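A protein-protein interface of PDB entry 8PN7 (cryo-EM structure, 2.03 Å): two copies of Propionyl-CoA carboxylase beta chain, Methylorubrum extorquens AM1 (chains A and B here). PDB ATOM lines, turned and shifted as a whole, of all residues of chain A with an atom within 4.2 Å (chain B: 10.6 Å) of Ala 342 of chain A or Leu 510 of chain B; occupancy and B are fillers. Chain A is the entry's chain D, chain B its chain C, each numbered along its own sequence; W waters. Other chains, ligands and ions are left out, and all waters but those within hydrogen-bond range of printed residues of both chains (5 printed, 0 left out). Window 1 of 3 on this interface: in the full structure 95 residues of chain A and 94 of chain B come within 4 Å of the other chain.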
ATOM      1  N   SER A 338      18.614 -11.774 -21.588  1.00  0.00           N
ATOM      2  CA  SER A 338      17.750 -11.069 -20.648  1.00  0.00           C
ATOM      3  C   SER A 338      16.281 -11.309 -20.969  1.00  0.00           C
ATOM      4  O   SER A 338      15.490 -11.632 -20.080  1.00  0.00           O
ATOM      5  CB  SER A 338      18.067  -9.573 -20.659  1.00  0.00           C
ATOM      6  OG  SER A 338      19.392  -9.327 -20.227  1.00  0.00           O
ATOM      7  N   ARG A 339      15.902 -11.176 -22.243  1.00  0.00           N
ATOM      8  CA  ARG A 339      14.507 -11.391 -22.623  1.00  0.00           C
ATOM      9  C   ARG A 339      14.082 -12.839 -22.402  1.00  0.00           C
ATOM     10  O   ARG A 339      12.979 -13.100 -21.903  1.00  0.00           O
ATOM     11  CB  ARG A 339      14.293 -10.976 -24.078  1.00  0.00           C
ATOM     12  CG  ARG A 339      14.387  -9.477 -24.306  1.00  0.00           C
ATOM     13  CD  ARG A 339      14.429  -9.116 -25.783  1.00  0.00           C
ATOM     14  NE  ARG A 339      13.271  -9.616 -26.513  1.00  0.00           N
ATOM     15  CZ  ARG A 339      13.319 -10.561 -27.441  1.00  0.00           C
ATOM     16  NH1 ARG A 339      14.463 -11.122 -27.798  1.00  0.00           N
ATOM     17  NH2 ARG A 339      12.194 -10.946 -28.032  1.00  0.00           N
ATOM     18  N   LYS A 340      14.943 -13.793 -22.766  1.00  0.00           N
ATOM     19  CA  LYS A 340      14.628 -15.205 -22.571  1.00  0.00           C
ATOM     20  C   LYS A 340      14.400 -15.524 -21.095  1.00  0.00           C
ATOM     21  O   LYS A 340      13.364 -16.092 -20.715  1.00  0.00           O
ATOM     22  CB  LYS A 340      15.758 -16.054 -23.156  1.00  0.00           C
ATOM     23  CG  LYS A 340      15.846 -17.482 -22.661  1.00  0.00           C
ATOM     24  CD  LYS A 340      17.035 -18.176 -23.308  1.00  0.00           C
ATOM     25  CE  LYS A 340      17.276 -19.554 -22.730  1.00  0.00           C
ATOM     26  NZ  LYS A 340      18.523 -20.151 -23.274  1.00  0.00           N
ATOM     27  N   ALA A 341      15.354 -15.139 -20.244  1.00  0.00           N
ATOM     28  CA  ALA A 341      15.230 -15.401 -18.816  1.00  0.00           C
ATOM     29  C   ALA A 341      14.043 -14.660 -18.218  1.00  0.00           C
ATOM     30  O   ALA A 341      13.367 -15.183 -17.328  1.00  0.00           O
ATOM     31  CB  ALA A 341      16.521 -15.017 -18.098  1.00  0.00           C
ATOM     32  N   ALA A 342      13.774 -13.441 -18.689  1.00  0.00           N
ATOM     33  CA  ALA A 342      12.659 -12.669 -18.158  1.00  0.00           C
ATOM     34  C   ALA A 342      11.332 -13.348 -18.458  1.00  0.00           C
ATOM     35  O   ALA A 342      10.474 -13.468 -17.577  1.00  0.00           O
ATOM     36  CB  ALA A 342      12.683 -11.252 -18.730  1.00  0.00           C
ATOM     37  N   ARG A 343      11.145 -13.805 -19.698  1.00  0.00           N
ATOM     38  CA  ARG A 343       9.909 -14.506 -20.030  1.00  0.00           C
ATOM     39  C   ARG A 343       9.772 -15.791 -19.223  1.00  0.00           C
ATOM     40  O   ARG A 343       8.679 -16.110 -18.733  1.00  0.00           O
ATOM     41  CB  ARG A 343       9.849 -14.809 -21.527  1.00  0.00           C
ATOM     42  CG  ARG A 343       8.518 -15.395 -21.983  1.00  0.00           C
ATOM     43  CD  ARG A 343       7.519 -14.301 -22.316  1.00  0.00           C
ATOM     44  NE  ARG A 343       6.167 -14.808 -22.523  1.00  0.00           N
ATOM     45  CZ  ARG A 343       5.729 -15.362 -23.646  1.00  0.00           C
ATOM     46  NH1 ARG A 343       6.525 -15.538 -24.686  1.00  0.00           N
ATOM     47  NH2 ARG A 343       4.460 -15.749 -23.726  1.00  0.00           N
ATOM     48  N   PHE A 344      10.870 -16.538 -19.063  1.00  0.00           N
ATOM     49  CA  PHE A 344      10.794 -17.774 -18.287  1.00  0.00           C
ATOM     50  C   PHE A 344      10.434 -17.497 -16.830  1.00  0.00           C
ATOM     51  O   PHE A 344       9.605 -18.201 -16.241  1.00  0.00           O
ATOM     52  CB  PHE A 344      12.114 -18.538 -18.380  1.00  0.00           C
ATOM     53  CG  PHE A 344      12.101 -19.857 -17.664  1.00  0.00           C
ATOM     54  CD1 PHE A 344      11.517 -20.969 -18.246  1.00  0.00           C
ATOM     55  CD2 PHE A 344      12.675 -19.987 -16.412  1.00  0.00           C
ATOM     56  CE1 PHE A 344      11.506 -22.184 -17.592  1.00  0.00           C
ATOM     57  CE2 PHE A 344      12.664 -21.200 -15.753  1.00  0.00           C
ATOM     58  CZ  PHE A 344      12.078 -22.300 -16.343  1.00  0.00           C
ATOM     59  N   VAL A 345      11.048 -16.472 -16.234  1.00  0.00           N
ATOM     60  CA  VAL A 345      10.765 -16.125 -14.844  1.00  0.00           C
ATOM     61  C   VAL A 345       9.323 -15.661 -14.693  1.00  0.00           C
ATOM     62  O   VAL A 345       8.648 -16.001 -13.715  1.00  0.00           O
ATOM     63  CB  VAL A 345      11.765 -15.063 -14.346  1.00  0.00           C
ATOM     64  CG1 VAL A 345      11.301 -14.456 -13.029  1.00  0.00           C
ATOM     65  CG2 VAL A 345      13.149 -15.674 -14.185  1.00  0.00           C
ATOM     66  N   ARG A 346       8.829 -14.875 -15.653  1.00  0.00           N
ATOM     67  CA  ARG A 346       7.441 -14.430 -15.601  1.00  0.00           C
ATOM     68  C   ARG A 346       6.484 -15.613 -15.667  1.00  0.00           C
ATOM     69  O   ARG A 346       5.498 -15.661 -14.922  1.00  0.00           O
ATOM     70  CB  ARG A 346       7.159 -13.448 -16.739  1.00  0.00           C
ATOM     71  CG  ARG A 346       7.868 -12.109 -16.608  1.00  0.00           C
ATOM     72  CD  ARG A 346       6.953 -11.041 -16.064  1.00  0.00           C
ATOM     73  NE  ARG A 346       5.830 -10.786 -16.956  1.00  0.00           N
ATOM     74  CZ  ARG A 346       4.915  -9.849 -16.759  1.00  0.00           C
ATOM     75  NH1 ARG A 346       4.962  -9.047 -15.708  1.00  0.00           N
ATOM     76  NH2 ARG A 346       3.927  -9.712 -17.638  1.00  0.00           N
ATOM     77  N   LYS A 381      14.033  -5.768 -18.241  1.00  0.00           N
ATOM     78  CA  LYS A 381      12.985  -6.785 -18.281  1.00  0.00           C
ATOM     79  C   LYS A 381      13.260  -7.902 -17.280  1.00  0.00           C
ATOM     80  O   LYS A 381      12.382  -8.282 -16.497  1.00  0.00           O
ATOM     81  CB  LYS A 381      12.852  -7.356 -19.693  1.00  0.00           C
ATOM     82  CG  LYS A 381      12.182  -6.439 -20.696  1.00  0.00           C
ATOM     83  CD  LYS A 381      12.116  -7.099 -22.062  1.00  0.00           C
ATOM     84  CE  LYS A 381      11.448  -6.207 -23.093  1.00  0.00           C
ATOM     85  NZ  LYS A 381      12.200  -4.944 -23.308  1.00  0.00           N
ATOM     86  N   LEU A 382      14.481  -8.445 -17.292  1.00  0.00           N
ATOM     87  CA  LEU A 382      14.829  -9.501 -16.347  1.00  0.00           C
ATOM     88  C   LEU A 382      14.843  -8.979 -14.916  1.00  0.00           C
ATOM     89  O   LEU A 382      14.384  -9.664 -13.991  1.00  0.00           O
ATOM     90  CB  LEU A 382      16.182 -10.111 -16.714  1.00  0.00           C
ATOM     91  CG  LEU A 382      16.708 -11.209 -15.788  1.00  0.00           C
ATOM     92  CD1 LEU A 382      15.720 -12.361 -15.688  1.00  0.00           C
ATOM     93  CD2 LEU A 382      18.065 -11.701 -16.262  1.00  0.00           C
ATOM     94  N   ALA A 385      11.216  -8.778 -13.875  1.00  0.00           N
ATOM     95  CA  ALA A 385      10.620 -10.091 -13.654  1.00  0.00           C
ATOM     96  C   ALA A 385      11.070 -10.683 -12.326  1.00  0.00           C
ATOM     97  O   ALA A 385      10.252 -11.223 -11.572  1.00  0.00           O
ATOM     98  CB  ALA A 385      10.969 -11.031 -14.807  1.00  0.00           C
ATOM     99  N   ILE A 508       5.799  -3.166 -17.273  1.00  0.00           N
ATOM    100  CA  ILE A 508       7.129  -3.694 -17.599  1.00  0.00           C
ATOM    101  C   ILE A 508       7.524  -3.236 -18.999  1.00  0.00           C
ATOM    102  O   ILE A 508       6.661  -3.175 -19.897  1.00  0.00           O
ATOM    103  CB  ILE A 508       7.141  -5.232 -17.491  1.00  0.00           C
ATOM    104  CG1 ILE A 508       8.541  -5.799 -17.732  1.00  0.00           C
ATOM    105  CG2 ILE A 508       6.143  -5.860 -18.460  1.00  0.00           C
ATOM    106  CD1 ILE A 508       8.621  -7.305 -17.613  1.00  0.00           C
ATOM    107  N   MET B 177      12.833   1.151 -15.923  1.00  0.00           N
ATOM    108  CA  MET B 177      11.601   0.564 -15.424  1.00  0.00           C
ATOM    109  C   MET B 177      10.532   1.606 -15.121  1.00  0.00           C
ATOM    110  O   MET B 177       9.418   1.235 -14.740  1.00  0.00           O
ATOM    111  CB  MET B 177      11.895  -0.280 -14.180  1.00  0.00           C
ATOM    112  CG  MET B 177      12.819  -1.460 -14.468  1.00  0.00           C
ATOM    113  SD  MET B 177      13.251  -2.430 -13.016  1.00  0.00           S
ATOM    114  CE  MET B 177      14.000  -1.169 -11.992  1.00  0.00           C
ATOM    115  N   SER B 222      14.776   2.913 -28.782  1.00  0.00           N
ATOM    116  CA  SER B 222      13.469   2.854 -28.126  1.00  0.00           C
ATOM    117  C   SER B 222      13.540   3.138 -26.630  1.00  0.00           C
ATOM    118  O   SER B 222      12.607   2.805 -25.895  1.00  0.00           O
ATOM    119  CB  SER B 222      12.775   1.505 -28.353  1.00  0.00           C
ATOM    120  OG  SER B 222      13.422   0.461 -27.649  1.00  0.00           O
ATOM    121  N   SER B 335       8.211  -3.969 -35.972  1.00  0.00           N
ATOM    122  CA  SER B 335       8.506  -4.294 -34.580  1.00  0.00           C
ATOM    123  C   SER B 335       8.592  -3.042 -33.715  1.00  0.00           C
ATOM    124  O   SER B 335       8.048  -3.008 -32.605  1.00  0.00           O
ATOM    125  CB  SER B 335       9.809  -5.089 -34.497  1.00  0.00           C
ATOM    126  OG  SER B 335       9.713  -6.301 -35.221  1.00  0.00           O
ATOM    127  N   ARG B 339       6.071  -2.209 -30.605  1.00  0.00           N
ATOM    128  CA  ARG B 339       6.512  -2.098 -29.216  1.00  0.00           C
ATOM    129  C   ARG B 339       6.173  -0.732 -28.627  1.00  0.00           C
ATOM    130  O   ARG B 339       5.717  -0.640 -27.478  1.00  0.00           O
ATOM    131  CB  ARG B 339       8.013  -2.372 -29.121  1.00  0.00           C
ATOM    132  CG  ARG B 339       8.386  -3.820 -29.391  1.00  0.00           C
ATOM    133  CD  ARG B 339       9.887  -4.012 -29.547  1.00  0.00           C
ATOM    134  NE  ARG B 339      10.633  -3.558 -28.381  1.00  0.00           N
ATOM    135  CZ  ARG B 339      11.455  -2.518 -28.374  1.00  0.00           C
ATOM    136  NH1 ARG B 339      11.681  -1.808 -29.467  1.00  0.00           N
ATOM    137  NH2 ARG B 339      12.071  -2.188 -27.244  1.00  0.00           N
ATOM    138  N   ALA B 342       2.442  -0.572 -28.066  1.00  0.00           N
ATOM    139  CA  ALA B 342       2.062  -1.506 -27.016  1.00  0.00           C
ATOM    140  C   ALA B 342       2.373  -0.939 -25.640  1.00  0.00           C
ATOM    141  O   ALA B 342       1.541  -1.004 -24.730  1.00  0.00           O
ATOM    142  CB  ALA B 342       2.771  -2.844 -27.223  1.00  0.00           C
ATOM    143  N   ARG B 343       3.570  -0.371 -25.469  1.00  0.00           N
ATOM    144  CA  ARG B 343       3.906   0.232 -24.183  1.00  0.00           C
ATOM    145  C   ARG B 343       2.981   1.401 -23.867  1.00  0.00           C
ATOM    146  O   ARG B 343       2.530   1.552 -22.724  1.00  0.00           O
ATOM    147  CB  ARG B 343       5.364   0.687 -24.168  1.00  0.00           C
ATOM    148  CG  ARG B 343       5.840   1.180 -22.808  1.00  0.00           C
ATOM    149  CD  ARG B 343       6.347   0.033 -21.950  1.00  0.00           C
ATOM    150  NE  ARG B 343       6.582   0.419 -20.563  1.00  0.00           N
ATOM    151  CZ  ARG B 343       7.668   1.043 -20.126  1.00  0.00           C
ATOM    152  NH1 ARG B 343       8.634   1.412 -20.949  1.00  0.00           N
ATOM    153  NH2 ARG B 343       7.786   1.306 -18.828  1.00  0.00           N
ATOM    154  N   ARG B 346      -0.418   0.011 -22.852  1.00  0.00           N
ATOM    155  CA  ARG B 346      -0.342  -0.578 -21.520  1.00  0.00           C
ATOM    156  C   ARG B 346      -0.331   0.498 -20.443  1.00  0.00           C
ATOM    157  O   ARG B 346      -1.010   0.366 -19.419  1.00  0.00           O
ATOM    158  CB  ARG B 346       0.898  -1.467 -21.406  1.00  0.00           C
ATOM    159  CG  ARG B 346       0.840  -2.738 -22.242  1.00  0.00           C
ATOM    160  CD  ARG B 346       0.468  -3.942 -21.408  1.00  0.00           C
ATOM    161  NE  ARG B 346       1.462  -4.208 -20.377  1.00  0.00           N
ATOM    162  CZ  ARG B 346       1.432  -5.249 -19.558  1.00  0.00           C
ATOM    163  NH1 ARG B 346       0.472  -6.154 -19.628  1.00  0.00           N
ATOM    164  NH2 ARG B 346       2.390  -5.385 -18.647  1.00  0.00           N
ATOM    165  N   GLY B 373      14.139 -10.390 -36.575  1.00  0.00           N
ATOM    166  CA  GLY B 373      14.056  -9.558 -35.397  1.00  0.00           C
ATOM    167  C   GLY B 373      12.923  -9.883 -34.456  1.00  0.00           C
ATOM    168  O   GLY B 373      12.796  -9.237 -33.415  1.00  0.00           O
ATOM    169  N   GLY B 374      12.095 -10.868 -34.786  1.00  0.00           N
ATOM    170  CA  GLY B 374      10.998 -11.245 -33.917  1.00  0.00           C
ATOM    171  C   GLY B 374       9.734 -10.441 -34.111  1.00  0.00           C
ATOM    172  O   GLY B 374       9.089 -10.062 -33.125  1.00  0.00           O
ATOM    173  N   LEU B 375       9.361 -10.160 -35.363  1.00  0.00           N
ATOM    174  CA  LEU B 375       8.154  -9.381 -35.627  1.00  0.00           C
ATOM    175  C   LEU B 375       6.903 -10.082 -35.114  1.00  0.00           C
ATOM    176  O   LEU B 375       5.929  -9.417 -34.746  1.00  0.00           O
ATOM    177  CB  LEU B 375       8.028  -9.097 -37.124  1.00  0.00           C
ATOM    178  CG  LEU B 375       6.743  -8.415 -37.603  1.00  0.00           C
ATOM    179  CD1 LEU B 375       6.587  -7.037 -36.980  1.00  0.00           C
ATOM    180  CD2 LEU B 375       6.708  -8.329 -39.118  1.00  0.00           C
ATOM    181  N   ILE B 376       6.910 -11.416 -35.074  1.00  0.00           N
ATOM    182  CA  ILE B 376       5.737 -12.151 -34.604  1.00  0.00           C
ATOM    183  C   ILE B 376       5.407 -11.764 -33.166  1.00  0.00           C
ATOM    184  O   ILE B 376       4.297 -11.307 -32.864  1.00  0.00           O
ATOM    185  CB  ILE B 376       5.971 -13.666 -34.752  1.00  0.00           C
ATOM    186  CG1 ILE B 376       6.218 -14.026 -36.218  1.00  0.00           C
ATOM    187  CG2 ILE B 376       4.791 -14.447 -34.222  1.00  0.00           C
ATOM    188  CD1 ILE B 376       6.568 -15.479 -36.447  1.00  0.00           C
ATOM    189  N   LYS B 377       6.392 -11.870 -32.270  1.00  0.00           N
ATOM    190  CA  LYS B 377       6.153 -11.528 -30.871  1.00  0.00           C
ATOM    191  C   LYS B 377       5.960 -10.030 -30.674  1.00  0.00           C
ATOM    192  O   LYS B 377       5.167  -9.617 -29.823  1.00  0.00           O
ATOM    193  CB  LYS B 377       7.299 -12.036 -29.997  1.00  0.00           C
ATOM    194  CG  LYS B 377       7.165 -13.498 -29.599  1.00  0.00           C
ATOM    195  CD  LYS B 377       8.271 -13.930 -28.651  1.00  0.00           C
ATOM    196  CE  LYS B 377       8.124 -15.396 -28.275  1.00  0.00           C
ATOM    197  NZ  LYS B 377       9.200 -15.855 -27.354  1.00  0.00           N
ATOM    198  N   HIS B 378       6.660  -9.201 -31.447  1.00  0.00           N
ATOM    199  CA  HIS B 378       6.540  -7.758 -31.260  1.00  0.00           C
ATOM    200  C   HIS B 378       5.165  -7.247 -31.677  1.00  0.00           C
ATOM    201  O   HIS B 378       4.582  -6.398 -30.993  1.00  0.00           O
ATOM    202  CB  HIS B 378       7.657  -7.047 -32.017  1.00  0.00           C
ATOM    203  CG  HIS B 378       9.018  -7.318 -31.457  1.00  0.00           C
ATOM    204  ND1 HIS B 378      10.149  -7.386 -32.240  1.00  0.00           N
ATOM    205  CD2 HIS B 378       9.425  -7.550 -30.188  1.00  0.00           C
ATOM    206  CE1 HIS B 378      11.196  -7.641 -31.477  1.00  0.00           C
ATOM    207  NE2 HIS B 378      10.784  -7.746 -30.227  1.00  0.00           N
ATOM    208  N   GLY B 379       4.628  -7.744 -32.793  1.00  0.00           N
ATOM    209  CA  GLY B 379       3.254  -7.420 -33.145  1.00  0.00           C
ATOM    210  C   GLY B 379       2.257  -8.023 -32.175  1.00  0.00           C
ATOM    211  O   GLY B 379       1.227  -7.407 -31.855  1.00  0.00           O
ATOM    212  N   ALA B 380       2.542  -9.236 -31.691  1.00  0.00           N
ATOM    213  CA  ALA B 380       1.707  -9.826 -30.657  1.00  0.00           C
ATOM    214  C   ALA B 380       1.687  -8.970 -29.400  1.00  0.00           C
ATOM    215  O   ALA B 380       0.720  -9.020 -28.645  1.00  0.00           O
ATOM    216  CB  ALA B 380       2.185 -11.238 -30.332  1.00  0.00           C
ATOM    217  N   LYS B 381       2.742  -8.192 -29.152  1.00  0.00           N
ATOM    218  CA  LYS B 381       2.743  -7.307 -27.990  1.00  0.00           C
ATOM    219  C   LYS B 381       1.636  -6.261 -28.090  1.00  0.00           C
ATOM    220  O   LYS B 381       0.888  -6.041 -27.133  1.00  0.00           O
ATOM    221  CB  LYS B 381       4.105  -6.630 -27.837  1.00  0.00           C
ATOM    222  CG  LYS B 381       5.208  -7.550 -27.365  1.00  0.00           C
ATOM    223  CD  LYS B 381       6.541  -6.833 -27.328  1.00  0.00           C
ATOM    224  CE  LYS B 381       7.665  -7.794 -27.005  1.00  0.00           C
ATOM    225  NZ  LYS B 381       8.968  -7.094 -26.870  1.00  0.00           N
ATOM    226  N   LEU B 382       1.520  -5.605 -29.246  1.00  0.00           N
ATOM    227  CA  LEU B 382       0.456  -4.622 -29.429  1.00  0.00           C
ATOM    228  C   LEU B 382      -0.914  -5.287 -29.424  1.00  0.00           C
ATOM    229  O   LEU B 382      -1.870  -4.755 -28.840  1.00  0.00           O
ATOM    230  CB  LEU B 382       0.675  -3.844 -30.726  1.00  0.00           C
ATOM    231  CG  LEU B 382      -0.385  -2.799 -31.081  1.00  0.00           C
ATOM    232  CD1 LEU B 382      -0.533  -1.772 -29.967  1.00  0.00           C
ATOM    233  CD2 LEU B 382      -0.042  -2.122 -32.397  1.00  0.00           C
ATOM    234  N   PHE B 384      -1.720  -7.983 -27.802  1.00  0.00           N
ATOM    235  CA  PHE B 384      -1.942  -8.325 -26.403  1.00  0.00           C
ATOM    236  C   PHE B 384      -2.365  -7.108 -25.597  1.00  0.00           C
ATOM    237  O   PHE B 384      -3.292  -7.184 -24.783  1.00  0.00           O
ATOM    238  CB  PHE B 384      -0.651  -8.926 -25.839  1.00  0.00           C
ATOM    239  CG  PHE B 384      -0.835  -9.751 -24.604  1.00  0.00           C
ATOM    240  CD1 PHE B 384      -1.062  -9.154 -23.377  1.00  0.00           C
ATOM    241  CD2 PHE B 384      -0.732 -11.130 -24.663  1.00  0.00           C
ATOM    242  CE1 PHE B 384      -1.214  -9.916 -22.241  1.00  0.00           C
ATOM    243  CE2 PHE B 384      -0.882 -11.896 -23.530  1.00  0.00           C
ATOM    244  CZ  PHE B 384      -1.122 -11.288 -22.317  1.00  0.00           C
ATOM    245  N   GLN B 388      -6.011  -6.782 -23.888  1.00  0.00           N
ATOM    246  CA  GLN B 388      -6.014  -6.749 -22.432  1.00  0.00           C
ATOM    247  C   GLN B 388      -6.718  -5.521 -21.867  1.00  0.00           C
ATOM    248  O   GLN B 388      -7.149  -5.549 -20.710  1.00  0.00           O
ATOM    249  CB  GLN B 388      -4.570  -6.801 -21.927  1.00  0.00           C
ATOM    250  CG  GLN B 388      -4.405  -7.087 -20.453  1.00  0.00           C
ATOM    251  CD  GLN B 388      -2.949  -7.098 -20.031  1.00  0.00           C
ATOM    252  OE1 GLN B 388      -2.098  -6.495 -20.682  1.00  0.00           O
ATOM    253  NE2 GLN B 388      -2.657  -7.790 -18.939  1.00  0.00           N
ATOM    254  N   HIS B 505      -0.331 -12.058 -12.880  1.00  0.00           N
ATOM    255  CA  HIS B 505      -0.086 -11.154 -13.993  1.00  0.00           C
ATOM    256  C   HIS B 505      -0.198 -11.977 -15.265  1.00  0.00           C
ATOM    257  O   HIS B 505      -0.260 -13.208 -15.227  1.00  0.00           O
ATOM    258  CB  HIS B 505       1.281 -10.467 -13.891  1.00  0.00           C
ATOM    259  CG  HIS B 505       2.429 -11.417 -13.750  1.00  0.00           C
ATOM    260  ND1 HIS B 505       2.830 -12.257 -14.767  1.00  0.00           N
ATOM    261  CD2 HIS B 505       3.261 -11.662 -12.711  1.00  0.00           C
ATOM    262  CE1 HIS B 505       3.860 -12.976 -14.360  1.00  0.00           C
ATOM    263  NE2 HIS B 505       4.141 -12.634 -13.116  1.00  0.00           N
ATOM    264  N   ASP B 506      -0.224 -11.283 -16.394  1.00  0.00           N
ATOM    265  CA  ASP B 506      -0.265 -11.943 -17.686  1.00  0.00           C
ATOM    266  C   ASP B 506       1.131 -12.435 -18.067  1.00  0.00           C
ATOM    267  O   ASP B 506       2.119 -12.195 -17.368  1.00  0.00           O
ATOM    268  CB  ASP B 506      -0.824 -10.995 -18.742  1.00  0.00           C
ATOM    269  CG  ASP B 506      -0.054  -9.692 -18.811  1.00  0.00           C
ATOM    270  OD1 ASP B 506       1.056  -9.690 -19.376  1.00  0.00           O
ATOM    271  OD2 ASP B 506      -0.551  -8.672 -18.292  1.00  0.00           O
ATOM    272  N   ASN B 507       1.214 -13.127 -19.199  1.00  0.00           N
ATOM    273  CA  ASN B 507       2.486 -13.618 -19.713  1.00  0.00           C
ATOM    274  C   ASN B 507       2.751 -13.013 -21.086  1.00  0.00           C
ATOM    275  O   ASN B 507       3.066 -13.733 -22.038  1.00  0.00           O
ATOM    276  CB  ASN B 507       2.496 -15.147 -19.773  1.00  0.00           C
ATOM    277  CG  ASN B 507       3.896 -15.717 -19.937  1.00  0.00           C
ATOM    278  OD1 ASN B 507       4.885 -15.077 -19.585  1.00  0.00           O
ATOM    279  ND2 ASN B 507       3.983 -16.926 -20.476  1.00  0.00           N
ATOM    280  N   ILE B 508       2.587 -11.697 -21.197  1.00  0.00           N
ATOM    281  CA  ILE B 508       2.777 -11.003 -22.477  1.00  0.00           C
ATOM    282  C   ILE B 508       4.188 -11.268 -22.989  1.00  0.00           C
ATOM    283  O   ILE B 508       5.139 -11.323 -22.183  1.00  0.00           O
ATOM    284  CB  ILE B 508       2.515  -9.493 -22.316  1.00  0.00           C
ATOM    285  CG1 ILE B 508       2.595  -8.766 -23.660  1.00  0.00           C
ATOM    286  CG2 ILE B 508       3.487  -8.866 -21.318  1.00  0.00           C
ATOM    287  CD1 ILE B 508       2.322  -7.279 -23.568  1.00  0.00           C
ATOM    288  N   PRO B 509       4.385 -11.479 -24.291  1.00  0.00           N
ATOM    289  CA  PRO B 509       5.742 -11.703 -24.801  1.00  0.00           C
ATOM    290  C   PRO B 509       6.644 -10.506 -24.544  1.00  0.00           C
ATOM    291  O   PRO B 509       6.203  -9.356 -24.533  1.00  0.00           O
ATOM    292  CB  PRO B 509       5.525 -11.928 -26.301  1.00  0.00           C
ATOM    293  CG  PRO B 509       4.124 -12.390 -26.414  1.00  0.00           C
ATOM    294  CD  PRO B 509       3.364 -11.696 -25.328  1.00  0.00           C
ATOM    295  N   LEU B 510       7.922 -10.794 -24.331  1.00  0.00           N
ATOM    296  CA  LEU B 510       8.903  -9.759 -24.034  1.00  0.00           C
ATOM    297  C   LEU B 510       9.951  -9.671 -25.140  1.00  0.00           C
ATOM    298  O   LEU B 510       9.938 -10.450 -26.092  1.00  0.00           O
ATOM    299  CB  LEU B 510       9.573 -10.032 -22.686  1.00  0.00           C
ATOM    300  CG  LEU B 510       8.624 -10.131 -21.490  1.00  0.00           C
ATOM    301  CD1 LEU B 510       9.371 -10.553 -20.239  1.00  0.00           C
ATOM    302  CD2 LEU B 510       7.903  -8.812 -21.267  1.00  0.00           C
ATOM    303  OXT LEU B 510      10.831  -8.811 -25.115  1.00  0.00           O
HETATM  304  O   HOH W   1       5.495 -12.114 -19.672  1.00  0.00           O
HETATM  305  O   HOH W   2       9.273 -16.492 -24.954  1.00  0.00           O
HETATM  306  O   HOH W   3       1.852  -7.687 -16.755  1.00  0.00           O
HETATM  307  O   HOH W   4      10.429 -10.820 -30.478  1.00  0.00           O
HETATM  308  O   HOH W   5       4.069  -2.622 -20.042  1.00  0.00           O
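OD1 of Asp 506 of chain B is in salt-bridge range of NH2 of Arg 346 of chain A (3.4 Å). O of Asn 507 of chain B is in hydrogen-bond range of NH2 of Arg 343 of chain A (3.0 Å). The chain-end carboxylate of Leu 510 of chain B is in salt-bridge range of the guanidinium group of Arg 339 of chain A (2.9 Å).
NH1 of Arg 346 of chain B lies within salt-bridge range of OD2 of Asp 506 of chain B, at 3.0 Å. N of Ile 508 of chain B lies within hydrogen-bond range of OD1 of Asp 506 of chain B (3.1 Å).
Among the printed residues, merely in contact across the chains: Arg 346 of chain A with His 505 of chain B (3.2 Å), Lys 381 of chain A with Leu 510 of chain B (3.4 Å), Arg 343 of chain A with Ile 508 of chain B (3.6 Å), Ile 508 of chain A with Arg 343 of chain B (3.7 Å), Ala 342 of chain A with Leu 510 of chain B (3.7 Å), Arg 343 of chain A with Leu 510 of chain B (3.7 Å), Ile 508 of chain A with Arg 346 of chain B (3.8 Å), Arg 343 of chain A with Lys 377 of chain B (3.8 Å), Arg 346 of chain A with Ile 508 of chain B (3.8 Å), Arg 343 of chain A with Pro 509 of chain B (3.8 Å) and Arg 346 of chain A with Asn 507 of chain B (3.99 Å).
Ala 342 of chain A touches one residue of chain B. Arg 339 of chain A touches just one residue of chain B: Leu 510 (2.9 Å). Arg 343 of chain A touches just these residues of chain B: Lys 377, Asn 507, Ile 508, Pro 509 and Leu 510. No residue of chain B comes within 4 Å of Leu 382 of chain A. Of the printed residues of chain A, Asn 507 of chain B touches Arg 343 and Arg 346. Printed residues of chain A within 4 Å of His 505 of chain B: Arg 346 (3.2 Å). Of the printed residues of chain A, Pro 509 of chain B touches Arg 343. The nearest residue of chain B that does not touch Ala 342 of chain A is Asn 507 of chain B (6.2 Å). The nearest printed residue of chain A that does not touch Leu 510 of chain B is Ile 508 of chain A (4.02 Å).
Printed residues of chain B that touch a printed residue of chain A: Arg 343, Arg 346, Lys 377, His 505, Asp 506, Asn 507, Ile 508, Pro 509 and Leu 510. Hydrophobic or aromatic side chains of chain B within 4 Å of the printed part of chain A: His 505, Ile 508 and Leu 510. Along chain B the printed residues that touch a printed residue of chain A span positions 343 to 510. Of the 13 printed residues of chain A, 6 touch a printed residue of chain B. Among the printed residues, 14 pairs touch across the chains. Among the printed residues, Asp or Glu carboxylates within 4 Å of a Lys or Arg side-chain nitrogen of the other chain: Arg 346 of chain A with Asp 506 of chain B (3.4 Å).
Arg 343 of chain A touches Ile 508 of chain B, and with the chains exchanged Ile 508 of chain A touches Arg 343 of chain B. Arg 346 of chain A touches Ile 508 of chain B, and with the chains exchanged Ile 508 of chain A touches Arg 346 of chain B.
Water W4 lies within hydrogen-bond range of the guanidinium group (NH2) of Arg 339 of chain A (3.0 Å), the backbone carbonyl oxygen (O) of Gly 374 of chain B (3.1 Å) and a ring nitrogen (NE2) of His 378 of chain B (3.1 Å).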
